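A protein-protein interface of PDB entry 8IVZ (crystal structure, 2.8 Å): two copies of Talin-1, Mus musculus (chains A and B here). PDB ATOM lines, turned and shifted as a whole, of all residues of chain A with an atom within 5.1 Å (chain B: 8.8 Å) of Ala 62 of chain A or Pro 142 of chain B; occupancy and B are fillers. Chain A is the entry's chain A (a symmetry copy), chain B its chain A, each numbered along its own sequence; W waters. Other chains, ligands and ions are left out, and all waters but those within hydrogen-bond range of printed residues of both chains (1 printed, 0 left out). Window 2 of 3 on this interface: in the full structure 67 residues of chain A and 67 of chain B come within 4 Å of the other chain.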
ATOM      1  N   GLY A  57      28.880 -38.726 -30.215  1.00  0.00           N
ATOM      2  CA  GLY A  57      29.611 -37.513 -29.887  1.00  0.00           C
ATOM      3  C   GLY A  57      28.902 -36.250 -30.322  1.00  0.00           C
ATOM      4  O   GLY A  57      29.079 -35.194 -29.708  1.00  0.00           O
ATOM      5  N   ILE A  58      28.097 -36.331 -31.382  1.00  0.00           N
ATOM      6  CA  ILE A  58      27.337 -35.169 -31.831  1.00  0.00           C
ATOM      7  C   ILE A  58      26.277 -34.797 -30.802  1.00  0.00           C
ATOM      8  O   ILE A  58      26.115 -33.624 -30.446  1.00  0.00           O
ATOM      9  CB  ILE A  58      26.713 -35.436 -33.213  1.00  0.00           C
ATOM     10  CG1 ILE A  58      27.797 -35.511 -34.289  1.00  0.00           C
ATOM     11  CG2 ILE A  58      25.699 -34.361 -33.557  1.00  0.00           C
ATOM     12  CD1 ILE A  58      27.286 -35.966 -35.639  1.00  0.00           C
ATOM     13  N   SER A  59      25.546 -35.794 -30.301  1.00  0.00           N
ATOM     14  CA  SER A  59      24.477 -35.524 -29.346  1.00  0.00           C
ATOM     15  C   SER A  59      25.029 -35.085 -27.995  1.00  0.00           C
ATOM     16  O   SER A  59      24.523 -34.131 -27.393  1.00  0.00           O
ATOM     17  CB  SER A  59      23.593 -36.761 -29.186  1.00  0.00           C
ATOM     18  OG  SER A  59      22.672 -36.598 -28.122  1.00  0.00           O
ATOM     19  N   GLN A  60      26.067 -35.766 -27.504  1.00  0.00           N
ATOM     20  CA  GLN A  60      26.583 -35.466 -26.172  1.00  0.00           C
ATOM     21  C   GLN A  60      27.254 -34.099 -26.124  1.00  0.00           C
ATOM     22  O   GLN A  60      27.039 -33.332 -25.179  1.00  0.00           O
ATOM     23  CB  GLN A  60      27.556 -36.557 -25.727  1.00  0.00           C
ATOM     24  CG  GLN A  60      26.910 -37.916 -25.511  1.00  0.00           C
ATOM     25  CD  GLN A  60      25.900 -37.909 -24.381  1.00  0.00           C
ATOM     26  OE1 GLN A  60      24.713 -37.657 -24.594  1.00  0.00           O
ATOM     27  NE2 GLN A  60      26.366 -38.188 -23.169  1.00  0.00           N
ATOM     28  N   ASN A  61      28.069 -33.773 -27.129  1.00  0.00           N
ATOM     29  CA  ASN A  61      28.802 -32.512 -27.097  1.00  0.00           C
ATOM     30  C   ASN A  61      27.895 -31.320 -27.369  1.00  0.00           C
ATOM     31  O   ASN A  61      28.158 -30.219 -26.869  1.00  0.00           O
ATOM     32  CB  ASN A  61      29.960 -32.553 -28.092  1.00  0.00           C
ATOM     33  CG  ASN A  61      31.082 -33.465 -27.635  1.00  0.00           C
ATOM     34  OD1 ASN A  61      31.440 -33.484 -26.458  1.00  0.00           O
ATOM     35  ND2 ASN A  61      31.639 -34.233 -28.565  1.00  0.00           N
ATOM     36  N   ALA A  62      26.834 -31.508 -28.157  1.00  0.00           N
ATOM     37  CA  ALA A  62      25.826 -30.460 -28.269  1.00  0.00           C
ATOM     38  C   ALA A  62      25.062 -30.294 -26.962  1.00  0.00           C
ATOM     39  O   ALA A  62      24.656 -29.180 -26.616  1.00  0.00           O
ATOM     40  CB  ALA A  62      24.862 -30.769 -29.417  1.00  0.00           C
ATOM     41  N   LYS A  63      24.868 -31.389 -26.224  1.00  0.00           N
ATOM     42  CA  LYS A  63      24.212 -31.305 -24.923  1.00  0.00           C
ATOM     43  C   LYS A  63      25.119 -30.646 -23.891  1.00  0.00           C
ATOM     44  O   LYS A  63      24.658 -29.838 -23.076  1.00  0.00           O
ATOM     45  CB  LYS A  63      23.791 -32.704 -24.472  1.00  0.00           C
ATOM     46  CG  LYS A  63      23.613 -32.873 -22.973  1.00  0.00           C
ATOM     47  CD  LYS A  63      23.467 -34.346 -22.616  1.00  0.00           C
ATOM     48  CE  LYS A  63      23.408 -34.560 -21.112  1.00  0.00           C
ATOM     49  NZ  LYS A  63      23.343 -36.009 -20.766  1.00  0.00           N
ATOM     50  N   ASN A  64      26.411 -30.966 -23.917  1.00  0.00           N
ATOM     51  CA  ASN A  64      27.358 -30.474 -22.927  1.00  0.00           C
ATOM     52  C   ASN A  64      28.013 -29.156 -23.321  1.00  0.00           C
ATOM     53  O   ASN A  64      28.833 -28.638 -22.556  1.00  0.00           O
ATOM     54  CB  ASN A  64      28.442 -31.527 -22.675  1.00  0.00           C
ATOM     55  CG  ASN A  64      27.875 -32.831 -22.153  1.00  0.00           C
ATOM     56  OD1 ASN A  64      26.941 -32.838 -21.352  1.00  0.00           O
ATOM     57  ND2 ASN A  64      28.434 -33.946 -22.613  1.00  0.00           N
ATOM     58  N   GLY A  65      27.677 -28.600 -24.483  1.00  0.00           N
ATOM     59  CA  GLY A  65      28.307 -27.370 -24.914  1.00  0.00           C
ATOM     60  C   GLY A  65      29.779 -27.492 -25.228  1.00  0.00           C
ATOM     61  O   GLY A  65      30.490 -26.484 -25.230  1.00  0.00           O
ATOM     62  N   PHE A  70      32.555 -31.320 -30.438  1.00  0.00           N
ATOM     63  CA  PHE A  70      31.380 -31.422 -31.296  1.00  0.00           C
ATOM     64  C   PHE A  70      31.766 -31.319 -32.764  1.00  0.00           C
ATOM     65  O   PHE A  70      31.275 -32.090 -33.597  1.00  0.00           O
ATOM     66  CB  PHE A  70      30.364 -30.341 -30.926  1.00  0.00           C
ATOM     67  CG  PHE A  70      29.222 -30.223 -31.898  1.00  0.00           C
ATOM     68  CD1 PHE A  70      28.150 -31.098 -31.840  1.00  0.00           C
ATOM     69  CD2 PHE A  70      29.219 -29.230 -32.864  1.00  0.00           C
ATOM     70  CE1 PHE A  70      27.098 -30.989 -32.733  1.00  0.00           C
ATOM     71  CE2 PHE A  70      28.172 -29.116 -33.760  1.00  0.00           C
ATOM     72  CZ  PHE A  70      27.109 -29.997 -33.693  1.00  0.00           C
ATOM     73  N   LEU B 131      19.923 -34.500 -39.824  1.00  0.00           N
ATOM     74  CA  LEU B 131      20.465 -34.656 -38.478  1.00  0.00           C
ATOM     75  C   LEU B 131      21.555 -33.627 -38.213  1.00  0.00           C
ATOM     76  O   LEU B 131      21.591 -33.010 -37.142  1.00  0.00           O
ATOM     77  CB  LEU B 131      20.997 -36.081 -38.290  1.00  0.00           C
ATOM     78  CG  LEU B 131      21.339 -36.578 -36.883  1.00  0.00           C
ATOM     79  CD1 LEU B 131      21.168 -38.087 -36.804  1.00  0.00           C
ATOM     80  CD2 LEU B 131      22.753 -36.192 -36.474  1.00  0.00           C
ATOM     81  N   THR B 134      19.933 -30.246 -37.880  1.00  0.00           N
ATOM     82  CA  THR B 134      19.327 -30.084 -36.563  1.00  0.00           C
ATOM     83  C   THR B 134      20.391 -29.922 -35.485  1.00  0.00           C
ATOM     84  O   THR B 134      20.252 -29.078 -34.591  1.00  0.00           O
ATOM     85  CB  THR B 134      18.423 -31.278 -36.254  1.00  0.00           C
ATOM     86  OG1 THR B 134      17.427 -31.402 -37.278  1.00  0.00           O
ATOM     87  CG2 THR B 134      17.735 -31.091 -34.912  1.00  0.00           C
ATOM     88  N   ALA B 135      21.465 -30.713 -35.557  1.00  0.00           N
ATOM     89  CA  ALA B 135      22.528 -30.612 -34.562  1.00  0.00           C
ATOM     90  C   ALA B 135      23.243 -29.270 -34.631  1.00  0.00           C
ATOM     91  O   ALA B 135      23.787 -28.807 -33.622  1.00  0.00           O
ATOM     92  CB  ALA B 135      23.527 -31.754 -34.742  1.00  0.00           C
ATOM     93  N   ARG B 136      23.256 -28.636 -35.805  1.00  0.00           N
ATOM     94  CA  ARG B 136      23.888 -27.327 -35.934  1.00  0.00           C
ATOM     95  C   ARG B 136      23.187 -26.290 -35.066  1.00  0.00           C
ATOM     96  O   ARG B 136      23.836 -25.416 -34.481  1.00  0.00           O
ATOM     97  CB  ARG B 136      23.892 -26.896 -37.401  1.00  0.00           C
ATOM     98  CG  ARG B 136      24.445 -25.504 -37.656  1.00  0.00           C
ATOM     99  CD  ARG B 136      24.332 -25.159 -39.129  1.00  0.00           C
ATOM    100  NE  ARG B 136      22.964 -25.332 -39.611  1.00  0.00           N
ATOM    101  CZ  ARG B 136      22.618 -25.347 -40.894  1.00  0.00           C
ATOM    102  NH1 ARG B 136      23.543 -25.204 -41.834  1.00  0.00           N
ATOM    103  NH2 ARG B 136      21.348 -25.511 -41.237  1.00  0.00           N
ATOM    104  N   ALA B 137      21.859 -26.375 -34.964  1.00  0.00           N
ATOM    105  CA  ALA B 137      21.125 -25.449 -34.110  1.00  0.00           C
ATOM    106  C   ALA B 137      21.199 -25.862 -32.645  1.00  0.00           C
ATOM    107  O   ALA B 137      21.285 -25.002 -31.762  1.00  0.00           O
ATOM    108  CB  ALA B 137      19.670 -25.352 -34.568  1.00  0.00           C
ATOM    109  N   LEU B 138      21.169 -27.168 -32.370  1.00  0.00           N
ATOM    110  CA  LEU B 138      21.286 -27.632 -30.991  1.00  0.00           C
ATOM    111  C   LEU B 138      22.652 -27.308 -30.404  1.00  0.00           C
ATOM    112  O   LEU B 138      22.780 -27.146 -29.185  1.00  0.00           O
ATOM    113  CB  LEU B 138      21.019 -29.136 -30.915  1.00  0.00           C
ATOM    114  CG  LEU B 138      19.576 -29.576 -31.153  1.00  0.00           C
ATOM    115  CD1 LEU B 138      19.470 -31.091 -31.134  1.00  0.00           C
ATOM    116  CD2 LEU B 138      18.656 -28.961 -30.111  1.00  0.00           C
ATOM    117  N   ALA B 139      23.683 -27.213 -31.248  1.00  0.00           N
ATOM    118  CA  ALA B 139      25.000 -26.828 -30.754  1.00  0.00           C
ATOM    119  C   ALA B 139      25.002 -25.387 -30.261  1.00  0.00           C
ATOM    120  O   ALA B 139      25.660 -25.066 -29.265  1.00  0.00           O
ATOM    121  CB  ALA B 139      26.051 -27.024 -31.846  1.00  0.00           C
ATOM    122  N   VAL B 140      24.267 -24.508 -30.940  1.00  0.00           N
ATOM    123  CA  VAL B 140      24.169 -23.120 -30.504  1.00  0.00           C
ATOM    124  C   VAL B 140      23.217 -22.993 -29.322  1.00  0.00           C
ATOM    125  O   VAL B 140      23.538 -22.359 -28.311  1.00  0.00           O
ATOM    126  CB  VAL B 140      23.739 -22.221 -31.679  1.00  0.00           C
ATOM    127  CG1 VAL B 140      23.573 -20.782 -31.215  1.00  0.00           C
ATOM    128  CG2 VAL B 140      24.752 -22.310 -32.810  1.00  0.00           C
ATOM    129  N   ASN B 141      22.035 -23.601 -29.425  1.00  0.00           N
ATOM    130  CA  ASN B 141      21.018 -23.541 -28.375  1.00  0.00           C
ATOM    131  C   ASN B 141      20.485 -24.943 -28.113  1.00  0.00           C
ATOM    132  O   ASN B 141      19.552 -25.399 -28.790  1.00  0.00           O
ATOM    133  CB  ASN B 141      19.884 -22.593 -28.762  1.00  0.00           C
ATOM    134  CG  ASN B 141      18.859 -22.426 -27.656  1.00  0.00           C
ATOM    135  OD1 ASN B 141      19.148 -22.672 -26.484  1.00  0.00           O
ATOM    136  ND2 ASN B 141      17.654 -22.003 -28.022  1.00  0.00           N
ATOM    137  N   PRO B 142      21.047 -25.659 -27.132  1.00  0.00           N
ATOM    138  CA  PRO B 142      20.505 -26.984 -26.794  1.00  0.00           C
ATOM    139  C   PRO B 142      19.186 -26.929 -26.040  1.00  0.00           C
ATOM    140  O   PRO B 142      18.553 -27.979 -25.870  1.00  0.00           O
ATOM    141  CB  PRO B 142      21.612 -27.604 -25.935  1.00  0.00           C
ATOM    142  CG  PRO B 142      22.275 -26.440 -25.300  1.00  0.00           C
ATOM    143  CD  PRO B 142      22.228 -25.323 -26.317  1.00  0.00           C
ATOM    144  N   ARG B 143      18.748 -25.751 -25.591  1.00  0.00           N
ATOM    145  CA  ARG B 143      17.472 -25.607 -24.892  1.00  0.00           C
ATOM    146  C   ARG B 143      16.315 -25.573 -25.895  1.00  0.00           C
ATOM    147  O   ARG B 143      15.504 -24.648 -25.937  1.00  0.00           O
ATOM    148  CB  ARG B 143      17.489 -24.355 -24.026  1.00  0.00           C
ATOM    149  CG  ARG B 143      18.666 -24.269 -23.069  1.00  0.00           C
ATOM    150  CD  ARG B 143      18.222 -24.489 -21.636  1.00  0.00           C
ATOM    151  NE  ARG B 143      17.084 -23.641 -21.293  1.00  0.00           N
ATOM    152  CZ  ARG B 143      17.187 -22.390 -20.858  1.00  0.00           C
ATOM    153  NH1 ARG B 143      16.096 -21.692 -20.572  1.00  0.00           N
ATOM    154  NH2 ARG B 143      18.381 -21.833 -20.711  1.00  0.00           N
ATOM    155  N   ASP B 144      16.251 -26.623 -26.712  1.00  0.00           N
ATOM    156  CA  ASP B 144      15.272 -26.724 -27.792  1.00  0.00           C
ATOM    157  C   ASP B 144      14.683 -28.127 -27.783  1.00  0.00           C
ATOM    158  O   ASP B 144      15.149 -29.016 -28.507  1.00  0.00           O
ATOM    159  CB  ASP B 144      15.911 -26.413 -29.147  1.00  0.00           C
ATOM    160  CG  ASP B 144      14.896 -25.996 -30.192  1.00  0.00           C
ATOM    161  OD1 ASP B 144      15.148 -24.995 -30.896  1.00  0.00           O
ATOM    162  OD2 ASP B 144      13.842 -26.655 -30.300  1.00  0.00           O
ATOM    163  N   PRO B 145      13.664 -28.367 -26.962  1.00  0.00           N
ATOM    164  CA  PRO B 145      13.050 -29.704 -26.897  1.00  0.00           C
ATOM    165  C   PRO B 145      12.518 -30.172 -28.244  1.00  0.00           C
ATOM    166  O   PRO B 145      12.698 -31.350 -28.589  1.00  0.00           O
ATOM    167  CB  PRO B 145      11.920 -29.525 -25.870  1.00  0.00           C
ATOM    168  CG  PRO B 145      12.398 -28.416 -24.997  1.00  0.00           C
ATOM    169  CD  PRO B 145      13.170 -27.481 -25.893  1.00  0.00           C
ATOM    170  N   PRO B 146      11.850 -29.315 -29.040  1.00  0.00           N
ATOM    171  CA  PRO B 146      11.373 -29.808 -30.347  1.00  0.00           C
ATOM    172  C   PRO B 146      12.480 -30.292 -31.269  1.00  0.00           C
ATOM    173  O   PRO B 146      12.290 -31.287 -31.979  1.00  0.00           O
ATOM    174  CB  PRO B 146      10.639 -28.593 -30.931  1.00  0.00           C
ATOM    175  CG  PRO B 146      10.189 -27.839 -29.753  1.00  0.00           C
ATOM    176  CD  PRO B 146      11.313 -27.965 -28.773  1.00  0.00           C
ATOM    177  N   ARG B 147      13.634 -29.621 -31.285  1.00  0.00           N
ATOM    178  CA  ARG B 147      14.698 -30.036 -32.194  1.00  0.00           C
ATOM    179  C   ARG B 147      15.348 -31.340 -31.751  1.00  0.00           C
ATOM    180  O   ARG B 147      15.787 -32.125 -32.598  1.00  0.00           O
ATOM    181  CB  ARG B 147      15.745 -28.932 -32.328  1.00  0.00           C
ATOM    182  CG  ARG B 147      15.360 -27.858 -33.330  1.00  0.00           C
ATOM    183  CD  ARG B 147      16.553 -27.007 -33.711  1.00  0.00           C
ATOM    184  NE  ARG B 147      16.228 -26.071 -34.783  1.00  0.00           N
ATOM    185  CZ  ARG B 147      15.737 -24.853 -34.584  1.00  0.00           C
ATOM    186  NH1 ARG B 147      15.470 -24.067 -35.618  1.00  0.00           N
ATOM    187  NH2 ARG B 147      15.512 -24.420 -33.351  1.00  0.00           N
ATOM    188  N   TRP B 148      15.422 -31.591 -30.442  1.00  0.00           N
ATOM    189  CA  TRP B 148      15.902 -32.890 -29.983  1.00  0.00           C
ATOM    190  C   TRP B 148      14.988 -34.013 -30.451  1.00  0.00           C
ATOM    191  O   TRP B 148      15.452 -35.135 -30.687  1.00  0.00           O
ATOM    192  CB  TRP B 148      16.032 -32.903 -28.459  1.00  0.00           C
ATOM    193  CG  TRP B 148      17.245 -32.181 -27.954  1.00  0.00           C
ATOM    194  CD1 TRP B 148      17.279 -30.965 -27.337  1.00  0.00           C
ATOM    195  CD2 TRP B 148      18.604 -32.630 -28.030  1.00  0.00           C
ATOM    196  NE1 TRP B 148      18.573 -30.630 -27.020  1.00  0.00           N
ATOM    197  CE2 TRP B 148      19.406 -31.636 -27.435  1.00  0.00           C
ATOM    198  CE3 TRP B 148      19.219 -33.777 -28.541  1.00  0.00           C
ATOM    199  CZ2 TRP B 148      20.792 -31.753 -27.338  1.00  0.00           C
ATOM    200  CZ3 TRP B 148      20.595 -33.892 -28.443  1.00  0.00           C
ATOM    201  CH2 TRP B 148      21.365 -32.886 -27.848  1.00  0.00           C
ATOM    202  N   LEU B 151      15.992 -34.314 -34.108  1.00  0.00           N
ATOM    203  CA  LEU B 151      17.255 -35.041 -34.174  1.00  0.00           C
ATOM    204  C   LEU B 151      17.042 -36.530 -33.939  1.00  0.00           C
ATOM    205  O   LEU B 151      17.635 -37.368 -34.630  1.00  0.00           O
ATOM    206  CB  LEU B 151      18.239 -34.472 -33.151  1.00  0.00           C
ATOM    207  CG  LEU B 151      19.692 -34.929 -33.271  1.00  0.00           C
ATOM    208  CD1 LEU B 151      20.430 -34.099 -34.308  1.00  0.00           C
ATOM    209  CD2 LEU B 151      20.397 -34.867 -31.925  1.00  0.00           C
HETATM  210  O   HOH W   1      25.837 -26.561 -26.971  1.00  0.00           O
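NE1 of Trp 148 of chain B is in hydrogen-bond range of O of Pro 142 of chain B (2.9 Å).
Ile 58 of chain A touches Ala 135 of chain B. O of Ser 59 of chain A touches CH2 of Trp 148 of chain B (3.4 Å). O of Ala 62 of chain A touches O of Leu 138 of chain B, at 3.8 Å. Ala 62 of chain A touches Pro 142 of chain B. Ala 135 of chain B touches Phe 70 of chain A (O to CZ, 3.5 Å). Phe 70 of chain A touches Ala 139 of chain B (CE2 to CB, 3.5 Å).
Of the printed residues of chain B, Ser 59 of chain A touches Trp 148. Of chain B, only Leu 138 and Pro 142 come within 4 Å of Ala 62 of chain A. Printed residues of chain A within 4 Å of Ala 135 of chain B: Ile 58 and Phe 70. Of the printed residues of chain A, Leu 138 of chain B touches Ala 62 (3.8 Å). Of the printed residues of chain A, Ala 139 of chain B touches Phe 70. Of the printed residues of chain A, Pro 142 of chain B touches Ala 62. Of the printed residues of chain A, Trp 148 of chain B touches Ser 59 (3.4 Å).
Of the 10 printed residues of chain A, 4 touch a printed residue of chain B. Hydrophobic or aromatic side chains of chain A that line the printed part of chain B: Ile 58 and Phe 70. Of the 17 printed residues of chain B, 5 touch a printed residue of chain A. Hydrophobic or aromatic side chains of chain B within 4 Å of the printed part of chain A: Ala 135, Ala 139, Pro 142 and Trp 148. Among the printed residues, no Asp or Glu carboxylate lies within 4 Å of a Lys or Arg side-chain nitrogen of the other chain.
No position is printed for both chains.
Water W1 lies within hydrogen-bond range of O of Ala 139 of chain B and O of Ala 62 of chain A.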
